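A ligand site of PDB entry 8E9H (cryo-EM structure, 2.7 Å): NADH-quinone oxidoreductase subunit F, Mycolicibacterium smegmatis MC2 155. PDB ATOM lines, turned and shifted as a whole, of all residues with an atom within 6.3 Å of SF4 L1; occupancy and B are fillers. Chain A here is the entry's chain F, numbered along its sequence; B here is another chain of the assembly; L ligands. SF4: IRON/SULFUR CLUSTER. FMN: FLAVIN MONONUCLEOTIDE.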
ATOM      1  N   ILE A 180       6.879 -24.322 -21.837  1.00  0.00           N
ATOM      2  CA  ILE A 180       6.315 -24.396 -23.177  1.00  0.00           C
ATOM      3  C   ILE A 180       7.391 -24.667 -24.216  1.00  0.00           C
ATOM      4  O   ILE A 180       7.125 -25.259 -25.264  1.00  0.00           O
ATOM      5  CB  ILE A 180       5.531 -23.117 -23.504  1.00  0.00           C
ATOM      6  CG1 ILE A 180       4.931 -23.187 -24.901  1.00  0.00           C
ATOM      7  CG2 ILE A 180       6.439 -21.900 -23.402  1.00  0.00           C
ATOM      8  CD1 ILE A 180       4.050 -24.390 -25.124  1.00  0.00           C
ATOM      9  N   GLN A 197       7.217 -19.541 -28.239  1.00  0.00           N
ATOM     10  CA  GLN A 197       5.799 -19.743 -28.451  1.00  0.00           C
ATOM     11  C   GLN A 197       5.560 -20.701 -29.613  1.00  0.00           C
ATOM     12  O   GLN A 197       6.270 -20.640 -30.620  1.00  0.00           O
ATOM     13  CB  GLN A 197       5.109 -18.410 -28.744  1.00  0.00           C
ATOM     14  CG  GLN A 197       5.274 -17.384 -27.657  1.00  0.00           C
ATOM     15  CD  GLN A 197       4.262 -16.281 -27.743  1.00  0.00           C
ATOM     16  OE1 GLN A 197       3.852 -15.893 -28.828  1.00  0.00           O
ATOM     17  NE2 GLN A 197       3.843 -15.765 -26.597  1.00  0.00           N
ATOM     18  N   PRO A 198       4.568 -21.575 -29.518  1.00  0.00           N
ATOM     19  CA  PRO A 198       4.332 -22.531 -30.608  1.00  0.00           C
ATOM     20  C   PRO A 198       4.025 -21.824 -31.922  1.00  0.00           C
ATOM     21  O   PRO A 198       3.449 -20.737 -31.949  1.00  0.00           O
ATOM     22  CB  PRO A 198       3.125 -23.342 -30.117  1.00  0.00           C
ATOM     23  CG  PRO A 198       3.149 -23.191 -28.651  1.00  0.00           C
ATOM     24  CD  PRO A 198       3.653 -21.818 -28.398  1.00  0.00           C
ATOM     25  N   GLU A 349       3.181 -21.003 -16.730  1.00  0.00           N
ATOM     26  CA  GLU A 349       3.915 -21.566 -17.850  1.00  0.00           C
ATOM     27  C   GLU A 349       3.281 -21.268 -19.198  1.00  0.00           C
ATOM     28  O   GLU A 349       3.937 -21.473 -20.231  1.00  0.00           O
ATOM     29  CB  GLU A 349       4.046 -23.083 -17.688  1.00  0.00           C
ATOM     30  N   SER A 350       2.033 -20.796 -19.241  1.00  0.00           N
ATOM     31  CA  SER A 350       1.412 -20.433 -20.508  1.00  0.00           C
ATOM     32  C   SER A 350       2.212 -19.334 -21.179  1.00  0.00           C
ATOM     33  O   SER A 350       2.585 -18.346 -20.536  1.00  0.00           O
ATOM     34  CB  SER A 350      -0.027 -19.973 -20.272  1.00  0.00           C
ATOM     35  OG  SER A 350      -0.852 -21.063 -19.928  1.00  0.00           O
ATOM     36  N   CYS A 351       2.461 -19.492 -22.478  1.00  0.00           N
ATOM     37  CA  CYS A 351       3.233 -18.458 -23.154  1.00  0.00           C
ATOM     38  C   CYS A 351       2.401 -17.194 -23.349  1.00  0.00           C
ATOM     39  O   CYS A 351       2.957 -16.104 -23.520  1.00  0.00           O
ATOM     40  CB  CYS A 351       3.748 -18.944 -24.506  1.00  0.00           C
ATOM     41  SG  CYS A 351       2.499 -19.281 -25.724  1.00  0.00           S
ATOM     42  N   GLY A 352       1.076 -17.306 -23.300  1.00  0.00           N
ATOM     43  CA  GLY A 352       0.190 -16.179 -23.418  1.00  0.00           C
ATOM     44  C   GLY A 352      -0.352 -15.952 -24.811  1.00  0.00           C
ATOM     45  O   GLY A 352      -1.220 -15.095 -24.985  1.00  0.00           O
ATOM     46  N   LYS A 353       0.123 -16.692 -25.814  1.00  0.00           N
ATOM     47  CA  LYS A 353      -0.362 -16.480 -27.169  1.00  0.00           C
ATOM     48  C   LYS A 353      -1.868 -16.688 -27.262  1.00  0.00           C
ATOM     49  O   LYS A 353      -2.585 -15.871 -27.839  1.00  0.00           O
ATOM     50  CB  LYS A 353       0.371 -17.416 -28.130  1.00  0.00           C
ATOM     51  CG  LYS A 353      -0.297 -17.573 -29.489  1.00  0.00           C
ATOM     52  CD  LYS A 353       0.513 -18.434 -30.432  1.00  0.00           C
ATOM     53  CE  LYS A 353       1.569 -17.648 -31.153  1.00  0.00           C
ATOM     54  NZ  LYS A 353       2.093 -18.409 -32.313  1.00  0.00           N
ATOM     55  N   CYS A 354      -2.363 -17.778 -26.698  1.00  0.00           N
ATOM     56  CA  CYS A 354      -3.779 -18.097 -26.786  1.00  0.00           C
ATOM     57  C   CYS A 354      -4.608 -17.130 -25.949  1.00  0.00           C
ATOM     58  O   CYS A 354      -4.133 -16.559 -24.967  1.00  0.00           O
ATOM     59  CB  CYS A 354      -4.061 -19.500 -26.285  1.00  0.00           C
ATOM     60  SG  CYS A 354      -3.672 -20.786 -27.417  1.00  0.00           S
ATOM     61  N   THR A 355      -5.859 -16.966 -26.356  1.00  0.00           N
ATOM     62  CA  THR A 355      -6.850 -16.495 -25.397  1.00  0.00           C
ATOM     63  C   THR A 355      -7.317 -17.638 -24.501  1.00  0.00           C
ATOM     64  O   THR A 355      -7.322 -17.462 -23.275  1.00  0.00           O
ATOM     65  CB  THR A 355      -8.032 -15.843 -26.131  1.00  0.00           C
ATOM     66  OG1 THR A 355      -7.538 -14.861 -27.041  1.00  0.00           O
ATOM     67  CG2 THR A 355      -8.966 -15.198 -25.138  1.00  0.00           C
ATOM     68  N   PRO A 356      -7.683 -18.804 -25.033  1.00  0.00           N
ATOM     69  CA  PRO A 356      -8.115 -19.886 -24.127  1.00  0.00           C
ATOM     70  C   PRO A 356      -7.099 -20.189 -23.041  1.00  0.00           C
ATOM     71  O   PRO A 356      -7.403 -19.998 -21.867  1.00  0.00           O
ATOM     72  CB  PRO A 356      -8.319 -21.064 -25.077  1.00  0.00           C
ATOM     73  CG  PRO A 356      -8.642 -20.449 -26.357  1.00  0.00           C
ATOM     74  CD  PRO A 356      -7.809 -19.215 -26.434  1.00  0.00           C
ATOM     75  N   CYS A 357      -5.894 -20.604 -23.399  1.00  0.00           N
ATOM     76  CA  CYS A 357      -4.956 -21.004 -22.360  1.00  0.00           C
ATOM     77  C   CYS A 357      -4.685 -19.859 -21.397  1.00  0.00           C
ATOM     78  O   CYS A 357      -4.895 -19.994 -20.181  1.00  0.00           O
ATOM     79  CB  CYS A 357      -3.659 -21.513 -22.981  1.00  0.00           C
ATOM     80  SG  CYS A 357      -2.301 -21.738 -21.825  1.00  0.00           S
ATOM     81  N   ARG A 358      -4.290 -18.704 -21.907  1.00  0.00           N
ATOM     82  CA  ARG A 358      -3.943 -17.591 -21.034  1.00  0.00           C
ATOM     83  C   ARG A 358      -5.078 -17.249 -20.088  1.00  0.00           C
ATOM     84  O   ARG A 358      -4.982 -17.427 -18.866  1.00  0.00           O
ATOM     85  CB  ARG A 358      -3.555 -16.371 -21.880  1.00  0.00           C
ATOM     86  CG  ARG A 358      -3.364 -15.103 -21.074  1.00  0.00           C
ATOM     87  CD  ARG A 358      -2.903 -13.943 -21.930  1.00  0.00           C
ATOM     88  NE  ARG A 358      -3.235 -14.104 -23.339  1.00  0.00           N
ATOM     89  CZ  ARG A 358      -4.272 -13.531 -23.942  1.00  0.00           C
ATOM     90  NH1 ARG A 358      -5.149 -12.796 -23.281  1.00  0.00           N
ATOM     91  NH2 ARG A 358      -4.437 -13.715 -25.249  1.00  0.00           N
ATOM     92  N   SER A 395      -7.445 -24.268 -27.542  1.00  0.00           N
ATOM     93  CA  SER A 395      -6.189 -23.541 -27.440  1.00  0.00           C
ATOM     94  C   SER A 395      -5.294 -23.852 -28.638  1.00  0.00           C
ATOM     95  O   SER A 395      -5.509 -24.802 -29.384  1.00  0.00           O
ATOM     96  CB  SER A 395      -5.479 -23.891 -26.140  1.00  0.00           C
ATOM     97  OG  SER A 395      -4.961 -25.210 -26.186  1.00  0.00           O
ATOM     98  N   PHE A 396      -4.269 -23.010 -28.799  1.00  0.00           N
ATOM     99  CA  PHE A 396      -3.408 -23.101 -29.970  1.00  0.00           C
ATOM    100  C   PHE A 396      -2.512 -24.327 -29.932  1.00  0.00           C
ATOM    101  O   PHE A 396      -2.327 -24.988 -30.956  1.00  0.00           O
ATOM    102  CB  PHE A 396      -2.563 -21.829 -30.077  1.00  0.00           C
ATOM    103  CG  PHE A 396      -1.720 -21.757 -31.300  1.00  0.00           C
ATOM    104  CD1 PHE A 396      -2.232 -21.230 -32.465  1.00  0.00           C
ATOM    105  CD2 PHE A 396      -0.407 -22.162 -31.267  1.00  0.00           C
ATOM    106  CE1 PHE A 396      -1.454 -21.142 -33.586  1.00  0.00           C
ATOM    107  CE2 PHE A 396       0.371 -22.073 -32.388  1.00  0.00           C
ATOM    108  CZ  PHE A 396      -0.150 -21.565 -33.552  1.00  0.00           C
ATOM    109  N   CYS A 397      -1.950 -24.644 -28.773  1.00  0.00           N
ATOM    110  CA  CYS A 397      -1.110 -25.825 -28.626  1.00  0.00           C
ATOM    111  C   CYS A 397      -1.677 -26.693 -27.520  1.00  0.00           C
ATOM    112  O   CYS A 397      -2.684 -26.354 -26.883  1.00  0.00           O
ATOM    113  CB  CYS A 397       0.347 -25.469 -28.312  1.00  0.00           C
ATOM    114  SG  CYS A 397       0.675 -25.155 -26.576  1.00  0.00           S
ATOM    115  N   ALA A 398      -1.030 -27.829 -27.294  1.00  0.00           N
ATOM    116  CA  ALA A 398      -1.548 -28.809 -26.350  1.00  0.00           C
ATOM    117  C   ALA A 398      -1.350 -28.410 -24.893  1.00  0.00           C
ATOM    118  O   ALA A 398      -1.826 -29.135 -24.023  1.00  0.00           O
ATOM    119  CB  ALA A 398      -0.895 -30.163 -26.608  1.00  0.00           C
ATOM    120  N   LEU A 399      -0.667 -27.305 -24.605  1.00  0.00           N
ATOM    121  CA  LEU A 399      -0.516 -26.907 -23.210  1.00  0.00           C
ATOM    122  C   LEU A 399      -1.869 -26.551 -22.593  1.00  0.00           C
ATOM    123  O   LEU A 399      -2.102 -26.822 -21.416  1.00  0.00           O
ATOM    124  CB  LEU A 399       0.433 -25.732 -23.083  1.00  0.00           C
ATOM    125  CG  LEU A 399       0.843 -25.419 -21.647  1.00  0.00           C
ATOM    126  CD1 LEU A 399       2.290 -24.970 -21.572  1.00  0.00           C
ATOM    127  CD2 LEU A 399      -0.058 -24.360 -21.035  1.00  0.00           C
ATOM    128  N   GLY A 400      -2.755 -25.939 -23.364  1.00  0.00           N
ATOM    129  CA  GLY A 400      -4.076 -25.626 -22.857  1.00  0.00           C
ATOM    130  C   GLY A 400      -4.834 -26.886 -22.516  1.00  0.00           C
ATOM    131  O   GLY A 400      -5.483 -26.975 -21.464  1.00  0.00           O
ATOM    132  N   ASP A 401      -4.761 -27.876 -23.397  1.00  0.00           N
ATOM    133  CA  ASP A 401      -5.404 -29.163 -23.125  1.00  0.00           C
ATOM    134  C   ASP A 401      -4.812 -29.793 -21.881  1.00  0.00           C
ATOM    135  O   ASP A 401      -5.529 -30.365 -21.053  1.00  0.00           O
ATOM    136  CB  ASP A 401      -5.259 -30.083 -24.336  1.00  0.00           C
ATOM    137  N   ALA B  58      -3.953 -16.661 -33.016  1.00  0.00           N
ATOM    138  CA  ALA B  58      -3.671 -16.475 -31.596  1.00  0.00           C
ATOM    139  C   ALA B  58      -4.951 -16.436 -30.773  1.00  0.00           C
ATOM    140  O   ALA B  58      -5.139 -17.238 -29.860  1.00  0.00           O
ATOM    141  CB  ALA B  58      -2.871 -15.198 -31.395  1.00  0.00           C
HETATM  142 FE1  SF4 L   1      -1.760 -21.044 -26.228  1.00  0.00          FE
HETATM  143 FE2  SF4 L   1      -0.052 -23.149 -25.897  1.00  0.00          FE
HETATM  144 FE3  SF4 L   1      -1.073 -21.838 -23.718  1.00  0.00          FE
HETATM  145 FE4  SF4 L   1       0.772 -20.619 -25.312  1.00  0.00          FE
HETATM  146  S1  SF4 L   1       1.084 -22.475 -24.043  1.00  0.00           S
HETATM  147  S2  SF4 L   1      -1.136 -19.702 -24.489  1.00  0.00           S
HETATM  148  S3  SF4 L   1       0.176 -21.419 -27.359  1.00  0.00           S
HETATM  149  S4  SF4 L   1      -2.233 -23.045 -25.264  1.00  0.00           S
HETATM  150  N1  FMN L   2       8.703 -33.376 -25.115  1.00  0.00           N
HETATM  151  C2  FMN L   2       9.916 -33.589 -24.486  1.00  0.00           C
HETATM  152  O2  FMN L   2      10.653 -34.498 -24.881  1.00  0.00           O
HETATM  153  N3  FMN L   2      10.299 -32.809 -23.422  1.00  0.00           N
HETATM  154  C4  FMN L   2       9.477 -31.799 -22.989  1.00  0.00           C
HETATM  155  O4  FMN L   2       9.805 -31.087 -22.041  1.00  0.00           O
HETATM  156  C4A FMN L   2       8.263 -31.575 -23.610  1.00  0.00           C
HETATM  157  N5  FMN L   2       7.449 -30.568 -23.172  1.00  0.00           N
HETATM  158  C5A FMN L   2       6.235 -30.344 -23.793  1.00  0.00           C
HETATM  159  C6  FMN L   2       5.424 -29.326 -23.333  1.00  0.00           C
HETATM  160  C7  FMN L   2       4.200 -29.085 -23.930  1.00  0.00           C
HETATM  161  C7M FMN L   2       3.355 -27.957 -23.406  1.00  0.00           C
HETATM  162  C8  FMN L   2       3.802 -29.869 -25.012  1.00  0.00           C
HETATM  163  C8M FMN L   2       2.499 -29.659 -25.703  1.00  0.00           C
HETATM  164  C9  FMN L   2       4.626 -30.893 -25.476  1.00  0.00           C
HETATM  165  C9A FMN L   2       5.848 -31.132 -24.856  1.00  0.00           C
HETATM  166  N10 FMN L   2       6.670 -32.154 -25.298  1.00  0.00           N
HETATM  167  C10 FMN L   2       7.876 -32.375 -24.681  1.00  0.00           C
HETATM  168  C1' FMN L   2       6.300 -33.035 -26.463  1.00  0.00           C
HETATM  169  C2' FMN L   2       6.877 -32.425 -27.716  1.00  0.00           C
HETATM  170  O2' FMN L   2       5.824 -32.013 -28.549  1.00  0.00           O
HETATM  171  C3' FMN L   2       7.811 -33.395 -28.446  1.00  0.00           C
HETATM  172  O3' FMN L   2       8.659 -32.667 -29.300  1.00  0.00           O
HETATM  173  C4' FMN L   2       7.040 -34.426 -29.260  1.00  0.00           C
HETATM  174  O4' FMN L   2       6.104 -35.077 -28.434  1.00  0.00           O
HETATM  175  C5' FMN L   2       7.974 -35.456 -29.863  1.00  0.00           C
HETATM  176  O5' FMN L   2       8.549 -36.223 -28.833  1.00  0.00           O
HETATM  177  P   FMN L   2       9.118 -37.693 -29.123  1.00  0.00           P
HETATM  178  O1P FMN L   2      10.601 -37.614 -29.359  1.00  0.00           O
HETATM  179  O2P FMN L   2       8.455 -38.260 -30.355  1.00  0.00           O
HETATM  180  O3P FMN L   2       8.859 -38.556 -27.931  1.00  0.00           O
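A sulfur (S1) of SF4 L1 lies close to the backbone NH of Cys 351, at 3.6 Å.
SG of Cys 351 is bound to FE4 of SF4 L1 (2.2 Å).
The side-chain sulfur (SG) of Cys 397 is bound to an iron atom (FE2) of SF4 L1.
The side-chain sulfur (SG) of Cys 357 binds an iron atom (FE3) of SF4 L1 (2.3 Å).
The backbone NH of Cys 354 lies close to a sulfur (S2) of SF4 L1.
FE1 of SF4 L1 is bound by SG of Cys 354 (2.3 Å).
A sulfur (S4) of SF4 L1 sits close to the side-chain hydroxyl of Ser 395, at 3.6 Å.
S2 of SF4 L1 lies close to N of Gly 352.
The backbone NH (N) of Gly 400 sits close to a sulfur (S4) of SF4 L1, at 3.5 Å.
N of Lys 353 sits close to S2 of SF4 L1.
The side-chain sulfur (SG) of Cys 351 lies close to the backbone NH (N) of Lys 353 (3.5 Å).
NE2 of Gln 197 is in hydrogen-bond range of O of Cys 351, 3.2 Å away.
The side-chain hydroxyl (OG) of Ser 395 sits at hydrogen-bond distance from the backbone carbonyl oxygen (O) of Cys 397.
The side-chain sulfur of Cys 357 sits close to the side-chain hydroxyl of Ser 350 (2.5 Å).
The side-chain sulfur (SG) of Cys 354 sits close to the backbone NH (N) of Phe 396, at 2.7 Å.
O of Cys 354 sits at hydrogen-bond distance from NH2 of Arg 358 (2.9 Å).
NE of Arg 358 lies within hydrogen-bond range of O of Gly 352 (2.8 Å).
The backbone carbonyl oxygen (O) of Pro 198 is in hydrogen-bond range of the side-chain amino group (NZ) of Lys 353.
Merely in contact with SF4 L1: Ile 180, Pro 198, Ser 350, Phe 396 and Leu 399.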
